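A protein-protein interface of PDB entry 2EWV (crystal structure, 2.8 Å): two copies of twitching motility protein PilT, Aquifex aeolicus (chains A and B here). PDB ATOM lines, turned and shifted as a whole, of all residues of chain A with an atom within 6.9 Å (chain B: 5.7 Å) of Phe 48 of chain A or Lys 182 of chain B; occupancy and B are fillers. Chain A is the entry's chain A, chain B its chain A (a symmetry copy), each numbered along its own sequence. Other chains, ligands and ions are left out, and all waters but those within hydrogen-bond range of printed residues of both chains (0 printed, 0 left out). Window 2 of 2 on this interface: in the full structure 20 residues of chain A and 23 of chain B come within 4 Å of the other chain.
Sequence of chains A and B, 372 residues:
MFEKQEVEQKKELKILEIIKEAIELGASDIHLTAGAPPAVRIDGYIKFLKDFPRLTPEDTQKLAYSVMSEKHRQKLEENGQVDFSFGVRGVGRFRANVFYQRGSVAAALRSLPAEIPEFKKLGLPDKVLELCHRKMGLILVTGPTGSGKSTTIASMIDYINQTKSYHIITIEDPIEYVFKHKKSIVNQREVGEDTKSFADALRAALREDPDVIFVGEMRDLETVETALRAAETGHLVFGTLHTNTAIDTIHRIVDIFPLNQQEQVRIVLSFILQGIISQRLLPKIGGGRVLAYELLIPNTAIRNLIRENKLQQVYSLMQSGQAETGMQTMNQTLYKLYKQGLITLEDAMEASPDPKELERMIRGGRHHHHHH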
ATOM      1  N   HIS A  31      13.486 -19.171  -1.693  1.00  0.00           N
ATOM      2  CA  HIS A  31      12.064 -19.528  -1.671  1.00  0.00           C
ATOM      3  C   HIS A  31      11.150 -18.306  -1.644  1.00  0.00           C
ATOM      4  O   HIS A  31      11.345 -17.385  -0.854  1.00  0.00           O
ATOM      5  CB  HIS A  31      11.755 -20.414  -0.456  1.00  0.00           C
ATOM      6  CG  HIS A  31      12.390 -21.776  -0.509  1.00  0.00           C
ATOM      7  ND1 HIS A  31      11.765 -22.871  -1.066  1.00  0.00           N
ATOM      8  CD2 HIS A  31      13.595 -22.216  -0.072  1.00  0.00           C
ATOM      9  CE1 HIS A  31      12.555 -23.925  -0.968  1.00  0.00           C
ATOM     10  NE2 HIS A  31      13.672 -23.555  -0.369  1.00  0.00           N
ATOM     11  N   THR A  33       7.366 -17.383  -1.021  1.00  0.00           N
ATOM     12  CA  THR A  33       6.084 -17.879  -0.560  1.00  0.00           C
ATOM     13  C   THR A  33       5.086 -16.725  -0.601  1.00  0.00           C
ATOM     14  O   THR A  33       5.302 -15.769  -1.334  1.00  0.00           O
ATOM     15  CB  THR A  33       6.225 -18.477   0.849  1.00  0.00           C
ATOM     16  OG1 THR A  33       5.016 -19.151   1.213  1.00  0.00           O
ATOM     17  CG2 THR A  33       6.544 -17.384   1.848  1.00  0.00           C
ATOM     18  N   ALA A  36       5.585 -14.371   3.608  1.00  0.00           N
ATOM     19  CA  ALA A  36       6.900 -13.858   3.921  1.00  0.00           C
ATOM     20  C   ALA A  36       7.520 -13.030   2.810  1.00  0.00           C
ATOM     21  O   ALA A  36       6.954 -12.909   1.723  1.00  0.00           O
ATOM     22  CB  ALA A  36       7.810 -15.026   4.263  1.00  0.00           C
ATOM     23  N   PRO A  37       8.677 -12.403   3.098  1.00  0.00           N
ATOM     24  CA  PRO A  37       9.426 -11.586   2.140  1.00  0.00           C
ATOM     25  C   PRO A  37      10.372 -12.620   1.510  1.00  0.00           C
ATOM     26  O   PRO A  37      10.839 -13.515   2.201  1.00  0.00           O
ATOM     27  CB  PRO A  37      10.146 -10.595   3.042  1.00  0.00           C
ATOM     28  CG  PRO A  37      10.467 -11.440   4.233  1.00  0.00           C
ATOM     29  CD  PRO A  37       9.185 -12.181   4.467  1.00  0.00           C
ATOM     30  N   PRO A  38      10.667 -12.523   0.207  1.00  0.00           N
ATOM     31  CA  PRO A  38      11.565 -13.552  -0.337  1.00  0.00           C
ATOM     32  C   PRO A  38      12.627 -14.102   0.619  1.00  0.00           C
ATOM     33  O   PRO A  38      13.418 -13.362   1.199  1.00  0.00           O
ATOM     34  CB  PRO A  38      12.150 -12.888  -1.586  1.00  0.00           C
ATOM     35  CG  PRO A  38      11.919 -11.425  -1.365  1.00  0.00           C
ATOM     36  CD  PRO A  38      10.577 -11.372  -0.703  1.00  0.00           C
ATOM     37  N   ALA A  39      12.618 -15.421   0.777  1.00  0.00           N
ATOM     38  CA  ALA A  39      13.536 -16.115   1.666  1.00  0.00           C
ATOM     39  C   ALA A  39      14.754 -16.692   0.953  1.00  0.00           C
ATOM     40  O   ALA A  39      14.818 -16.721  -0.276  1.00  0.00           O
ATOM     41  CB  ALA A  39      12.797 -17.217   2.384  1.00  0.00           C
ATOM     42  N   VAL A  40      15.704 -17.186   1.739  1.00  0.00           N
ATOM     43  CA  VAL A  40      16.941 -17.735   1.199  1.00  0.00           C
ATOM     44  C   VAL A  40      17.616 -18.770   2.119  1.00  0.00           C
ATOM     45  O   VAL A  40      17.784 -18.534   3.311  1.00  0.00           O
ATOM     46  CB  VAL A  40      17.904 -16.572   0.922  1.00  0.00           C
ATOM     47  CG1 VAL A  40      19.314 -17.051   0.923  1.00  0.00           C
ATOM     48  CG2 VAL A  40      17.566 -15.938  -0.396  1.00  0.00           C
ATOM     49  N   ILE A  46      17.236 -21.197   6.808  1.00  0.00           N
ATOM     50  CA  ILE A  46      16.272 -20.377   6.099  1.00  0.00           C
ATOM     51  C   ILE A  46      16.277 -18.991   6.724  1.00  0.00           C
ATOM     52  O   ILE A  46      15.910 -18.832   7.891  1.00  0.00           O
ATOM     53  CB  ILE A  46      14.836 -20.938   6.197  1.00  0.00           C
ATOM     54  CG1 ILE A  46      14.640 -22.035   5.156  1.00  0.00           C
ATOM     55  CG2 ILE A  46      13.819 -19.832   5.966  1.00  0.00           C
ATOM     56  CD1 ILE A  46      15.511 -23.238   5.384  1.00  0.00           C
ATOM     57  N   LYS A  47      16.714 -18.006   5.937  1.00  0.00           N
ATOM     58  CA  LYS A  47      16.760 -16.601   6.348  1.00  0.00           C
ATOM     59  C   LYS A  47      15.926 -15.765   5.381  1.00  0.00           C
ATOM     60  O   LYS A  47      16.111 -15.851   4.170  1.00  0.00           O
ATOM     61  CB  LYS A  47      18.193 -16.087   6.351  1.00  0.00           C
ATOM     62  CG  LYS A  47      18.711 -15.820   7.737  1.00  0.00           C
ATOM     63  CD  LYS A  47      19.182 -17.081   8.421  1.00  0.00           C
ATOM     64  CE  LYS A  47      20.705 -17.041   8.541  1.00  0.00           C
ATOM     65  NZ  LYS A  47      21.271 -18.017   9.526  1.00  0.00           N
ATOM     66  N   PHE A  48      15.010 -14.961   5.918  1.00  0.00           N
ATOM     67  CA  PHE A  48      14.131 -14.123   5.094  1.00  0.00           C
ATOM     68  C   PHE A  48      14.836 -12.808   4.758  1.00  0.00           C
ATOM     69  O   PHE A  48      15.001 -11.959   5.630  1.00  0.00           O
ATOM     70  CB  PHE A  48      12.806 -13.836   5.835  1.00  0.00           C
ATOM     71  CG  PHE A  48      12.116 -15.076   6.389  1.00  0.00           C
ATOM     72  CD1 PHE A  48      12.624 -15.734   7.511  1.00  0.00           C
ATOM     73  CD2 PHE A  48      10.979 -15.596   5.779  1.00  0.00           C
ATOM     74  CE1 PHE A  48      12.015 -16.890   8.015  1.00  0.00           C
ATOM     75  CE2 PHE A  48      10.365 -16.750   6.276  1.00  0.00           C
ATOM     76  CZ  PHE A  48      10.891 -17.396   7.397  1.00  0.00           C
ATOM     77  N   LEU A  49      15.250 -12.638   3.500  1.00  0.00           N
ATOM     78  CA  LEU A  49      15.952 -11.418   3.107  1.00  0.00           C
ATOM     79  C   LEU A  49      15.029 -10.220   2.963  1.00  0.00           C
ATOM     80  O   LEU A  49      14.451  -9.962   1.910  1.00  0.00           O
ATOM     81  CB  LEU A  49      16.786 -11.636   1.823  1.00  0.00           C
ATOM     82  CG  LEU A  49      16.254 -11.961   0.427  1.00  0.00           C
ATOM     83  CD1 LEU A  49      15.805 -10.718  -0.301  1.00  0.00           C
ATOM     84  CD2 LEU A  49      17.376 -12.579  -0.356  1.00  0.00           C
ATOM     85  N   LYS A  50      14.900  -9.493   4.065  1.00  0.00           N
ATOM     86  CA  LYS A  50      14.067  -8.305   4.130  1.00  0.00           C
ATOM     87  C   LYS A  50      14.876  -7.123   3.637  1.00  0.00           C
ATOM     88  O   LYS A  50      14.381  -5.998   3.583  1.00  0.00           O
ATOM     89  CB  LYS A  50      13.622  -8.078   5.574  1.00  0.00           C
ATOM     90  CG  LYS A  50      14.754  -8.210   6.576  1.00  0.00           C
ATOM     91  CD  LYS A  50      14.267  -8.846   7.863  1.00  0.00           C
ATOM     92  CE  LYS A  50      15.428  -9.154   8.788  1.00  0.00           C
ATOM     93  NZ  LYS A  50      14.979  -9.842  10.033  1.00  0.00           N
ATOM     94  N   ASP A  51      16.125  -7.407   3.277  1.00  0.00           N
ATOM     95  CA  ASP A  51      17.067  -6.410   2.779  1.00  0.00           C
ATOM     96  C   ASP A  51      16.386  -5.273   2.022  1.00  0.00           C
ATOM     97  O   ASP A  51      16.719  -4.103   2.218  1.00  0.00           O
ATOM     98  CB  ASP A  51      18.113  -7.082   1.883  1.00  0.00           C
ATOM     99  CG  ASP A  51      19.120  -7.922   2.671  1.00  0.00           C
ATOM    100  OD1 ASP A  51      19.788  -7.359   3.571  1.00  0.00           O
ATOM    101  OD2 ASP A  51      19.251  -9.138   2.389  1.00  0.00           O
ATOM    102  N   ASP B 158       4.206 -26.910  14.733  1.00  0.00           N
ATOM    103  CA  ASP B 158       4.288 -25.496  15.142  1.00  0.00           C
ATOM    104  C   ASP B 158       5.399 -25.181  16.153  1.00  0.00           C
ATOM    105  O   ASP B 158       5.876 -24.042  16.227  1.00  0.00           O
ATOM    106  CB  ASP B 158       2.964 -24.997  15.714  1.00  0.00           C
ATOM    107  CG  ASP B 158       2.912 -23.480  15.792  1.00  0.00           C
ATOM    108  OD1 ASP B 158       3.094 -22.847  14.733  1.00  0.00           O
ATOM    109  OD2 ASP B 158       2.690 -22.921  16.892  1.00  0.00           O
ATOM    110  N   ASN B 161       8.261 -24.780  13.745  1.00  0.00           N
ATOM    111  CA  ASN B 161       8.102 -23.505  13.071  1.00  0.00           C
ATOM    112  C   ASN B 161       8.551 -22.368  13.989  1.00  0.00           C
ATOM    113  O   ASN B 161       8.867 -21.264  13.531  1.00  0.00           O
ATOM    114  CB  ASN B 161       6.617 -23.346  12.651  1.00  0.00           C
ATOM    115  CG  ASN B 161       6.304 -21.981  12.025  1.00  0.00           C
ATOM    116  OD1 ASN B 161       7.127 -21.390  11.331  1.00  0.00           O
ATOM    117  ND2 ASN B 161       5.094 -21.495  12.261  1.00  0.00           N
ATOM    118  N   GLN B 162       8.592 -22.648  15.285  1.00  0.00           N
ATOM    119  CA  GLN B 162       8.977 -21.633  16.247  1.00  0.00           C
ATOM    120  C   GLN B 162      10.455 -21.615  16.587  1.00  0.00           C
ATOM    121  O   GLN B 162      11.067 -20.552  16.617  1.00  0.00           O
ATOM    122  CB  GLN B 162       8.138 -21.785  17.510  1.00  0.00           C
ATOM    123  CG  GLN B 162       6.677 -21.519  17.246  1.00  0.00           C
ATOM    124  CD  GLN B 162       5.845 -21.495  18.500  1.00  0.00           C
ATOM    125  OE1 GLN B 162       5.969 -22.369  19.365  1.00  0.00           O
ATOM    126  NE2 GLN B 162       4.971 -20.498  18.606  1.00  0.00           N
ATOM    127  N   PHE B 179      -0.864 -22.192   9.257  1.00  0.00           N
ATOM    128  CA  PHE B 179       0.368 -21.757   9.908  1.00  0.00           C
ATOM    129  C   PHE B 179       0.956 -20.380   9.529  1.00  0.00           C
ATOM    130  O   PHE B 179       1.085 -20.017   8.354  1.00  0.00           O
ATOM    131  CB  PHE B 179       1.466 -22.820   9.729  1.00  0.00           C
ATOM    132  CG  PHE B 179       1.078 -24.234  10.153  1.00  0.00           C
ATOM    133  CD1 PHE B 179       0.404 -25.083   9.280  1.00  0.00           C
ATOM    134  CD2 PHE B 179       1.506 -24.751  11.372  1.00  0.00           C
ATOM    135  CE1 PHE B 179       0.176 -26.426   9.608  1.00  0.00           C
ATOM    136  CE2 PHE B 179       1.283 -26.090  11.707  1.00  0.00           C
ATOM    137  CZ  PHE B 179       0.616 -26.926  10.817  1.00  0.00           C
ATOM    138  N   LYS B 180       1.331 -19.636  10.566  1.00  0.00           N
ATOM    139  CA  LYS B 180       1.928 -18.314  10.435  1.00  0.00           C
ATOM    140  C   LYS B 180       3.411 -18.485  10.206  1.00  0.00           C
ATOM    141  O   LYS B 180       4.062 -19.248  10.915  1.00  0.00           O
ATOM    142  CB  LYS B 180       1.746 -17.508  11.726  1.00  0.00           C
ATOM    143  CG  LYS B 180       0.360 -16.917  11.973  1.00  0.00           C
ATOM    144  CD  LYS B 180       0.375 -16.088  13.264  1.00  0.00           C
ATOM    145  CE  LYS B 180      -0.754 -15.044  13.325  1.00  0.00           C
ATOM    146  NZ  LYS B 180      -0.590 -14.069  14.463  1.00  0.00           N
ATOM    147  N   HIS B 181       3.952 -17.784   9.215  1.00  0.00           N
ATOM    148  CA  HIS B 181       5.390 -17.867   8.950  1.00  0.00           C
ATOM    149  C   HIS B 181       6.090 -17.322  10.195  1.00  0.00           C
ATOM    150  O   HIS B 181       5.893 -16.160  10.557  1.00  0.00           O
ATOM    151  CB  HIS B 181       5.798 -16.983   7.759  1.00  0.00           C
ATOM    152  CG  HIS B 181       5.280 -17.445   6.432  1.00  0.00           C
ATOM    153  ND1 HIS B 181       5.806 -18.528   5.761  1.00  0.00           N
ATOM    154  CD2 HIS B 181       4.314 -16.936   5.628  1.00  0.00           C
ATOM    155  CE1 HIS B 181       5.192 -18.664   4.601  1.00  0.00           C
ATOM    156  NE2 HIS B 181       4.283 -17.711   4.494  1.00  0.00           N
ATOM    157  N   LYS B 182       6.887 -18.145  10.862  1.00  0.00           N
ATOM    158  CA  LYS B 182       7.605 -17.661  12.031  1.00  0.00           C
ATOM    159  C   LYS B 182       9.122 -17.618  11.760  1.00  0.00           C
ATOM    160  O   LYS B 182       9.582 -16.774  10.985  1.00  0.00           O
ATOM    161  CB  LYS B 182       7.276 -18.516  13.257  1.00  0.00           C
ATOM    162  CG  LYS B 182       6.151 -17.943  14.139  1.00  0.00           C
ATOM    163  CD  LYS B 182       4.768 -18.420  13.756  1.00  0.00           C
ATOM    164  CE  LYS B 182       4.114 -19.106  14.943  1.00  0.00           C
ATOM    165  NZ  LYS B 182       2.708 -19.533  14.662  1.00  0.00           N
ATOM    166  N   LYS B 183       9.897 -18.504  12.381  1.00  0.00           N
ATOM    167  CA  LYS B 183      11.346 -18.535  12.164  1.00  0.00           C
ATOM    168  C   LYS B 183      11.600 -19.370  10.927  1.00  0.00           C
ATOM    169  O   LYS B 183      12.740 -19.571  10.514  1.00  0.00           O
ATOM    170  CB  LYS B 183      12.059 -19.177  13.359  1.00  0.00           C
ATOM    171  CG  LYS B 183      13.575 -18.935  13.435  1.00  0.00           C
ATOM    172  CD  LYS B 183      14.166 -19.527  14.715  1.00  0.00           C
ATOM    173  CE  LYS B 183      15.590 -19.040  14.963  1.00  0.00           C
ATOM    174  NZ  LYS B 183      15.640 -17.592  15.343  1.00  0.00           N
ATOM    175  N   SER B 184      10.516 -19.866  10.343  1.00  0.00           N
ATOM    176  CA  SER B 184      10.590 -20.689   9.144  1.00  0.00           C
ATOM    177  C   SER B 184       9.418 -20.423   8.185  1.00  0.00           C
ATOM    178  O   SER B 184       8.410 -19.828   8.554  1.00  0.00           O
ATOM    179  CB  SER B 184      10.664 -22.182   9.533  1.00  0.00           C
ATOM    180  OG  SER B 184       9.430 -22.685   9.979  1.00  0.00           O
ATOM    181  N   ILE B 185       9.587 -20.868   6.948  1.00  0.00           N
ATOM    182  CA  ILE B 185       8.605 -20.704   5.892  1.00  0.00           C
ATOM    183  C   ILE B 185       7.732 -21.975   5.691  1.00  0.00           C
ATOM    184  O   ILE B 185       8.220 -23.021   5.274  1.00  0.00           O
ATOM    185  CB  ILE B 185       9.360 -20.286   4.578  1.00  0.00           C
ATOM    186  CG1 ILE B 185       8.429 -20.311   3.368  1.00  0.00           C
ATOM    187  CG2 ILE B 185      10.554 -21.195   4.349  1.00  0.00           C
ATOM    188  CD1 ILE B 185       9.165 -20.141   2.036  1.00  0.00           C
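Ile 185 of chain B touches His 31 of chain A.
His 181 of chain B touches Thr 33 of chain A.
CB of Thr 33 of chain A touches CD1 of Ile 185 of chain B (3.6 Å).
His 181 of chain B touches Ala 36 of chain A.
CG2 of Ile 46 of chain A touches CG2 of Ile 185 of chain B, at 3.9 Å.
Phe 48 of chain A touches Lys 182 of chain B (CE1 to O, 3.8 Å).
Lys 183 of chain B touches Phe 48 of chain A (O to CE1, 3.7 Å).
Ser 184 of chain B touches Phe 48 of chain A (C to CZ, 3.5 Å).
N of Ile 185 of chain B touches CZ of Phe 48 of chain A (3.7 Å).
The backbone NH (N) of Lys 182 of chain B is in hydrogen-bond range of the side-chain amide oxygen (OD1) of Asn 161 of chain B, 3.3 Å away.
The backbone NH (N) of Lys 183 of chain B sits at hydrogen-bond distance from the backbone carbonyl oxygen (O) of Asn 161 of chain B (3.2 Å).
NZ of Lys 182 of chain B is in salt-bridge range of OD1 of Asp 158 of chain B (3.3 Å).
The side-chain amide oxygen (OD1) of Asn 161 of chain B sits at hydrogen-bond distance from the side-chain hydroxyl (OG) of Ser 184 of chain B (3.0 Å).
N of Ala 39 of chain A is in hydrogen-bond range of O of His 31 of chain A (2.9 Å).
No position is printed for both chains.
Of the 10 printed residues of chain B, 5 touch a printed residue of chain A.
Of the 13 printed residues of chain A, 5 touch a printed residue of chain B.
Printed residues of chain A that touch a printed residue of chain B: His 31, Thr 33, Ala 36, Ile 46 and Phe 48.
Among the printed residues, 9 pairs touch across the chains.
Phe 48 of chain A touches just these residues of chain B: Lys 182, Lys 183, Ser 184 and Ile 185.
Lys 182 of chain B touches just one residue of chain A: Phe 48 (3.8 Å).
Of the printed residues of chain B, His 31 of chain A touches Ile 185.
Printed residues of chain A within 4 Å of Ser 184 of chain B: Phe 48.
Of the printed residues of chain B, Ala 36 of chain A touches His 181.
Of the printed residues of chain B, Thr 33 of chain A touches His 181 and Ile 185.
Lys 47 of chain A touches none of the printed residues of chain B.
The nearest residue of chain B that does not touch Phe 48 of chain A is His 181 of chain B (4.8 Å).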
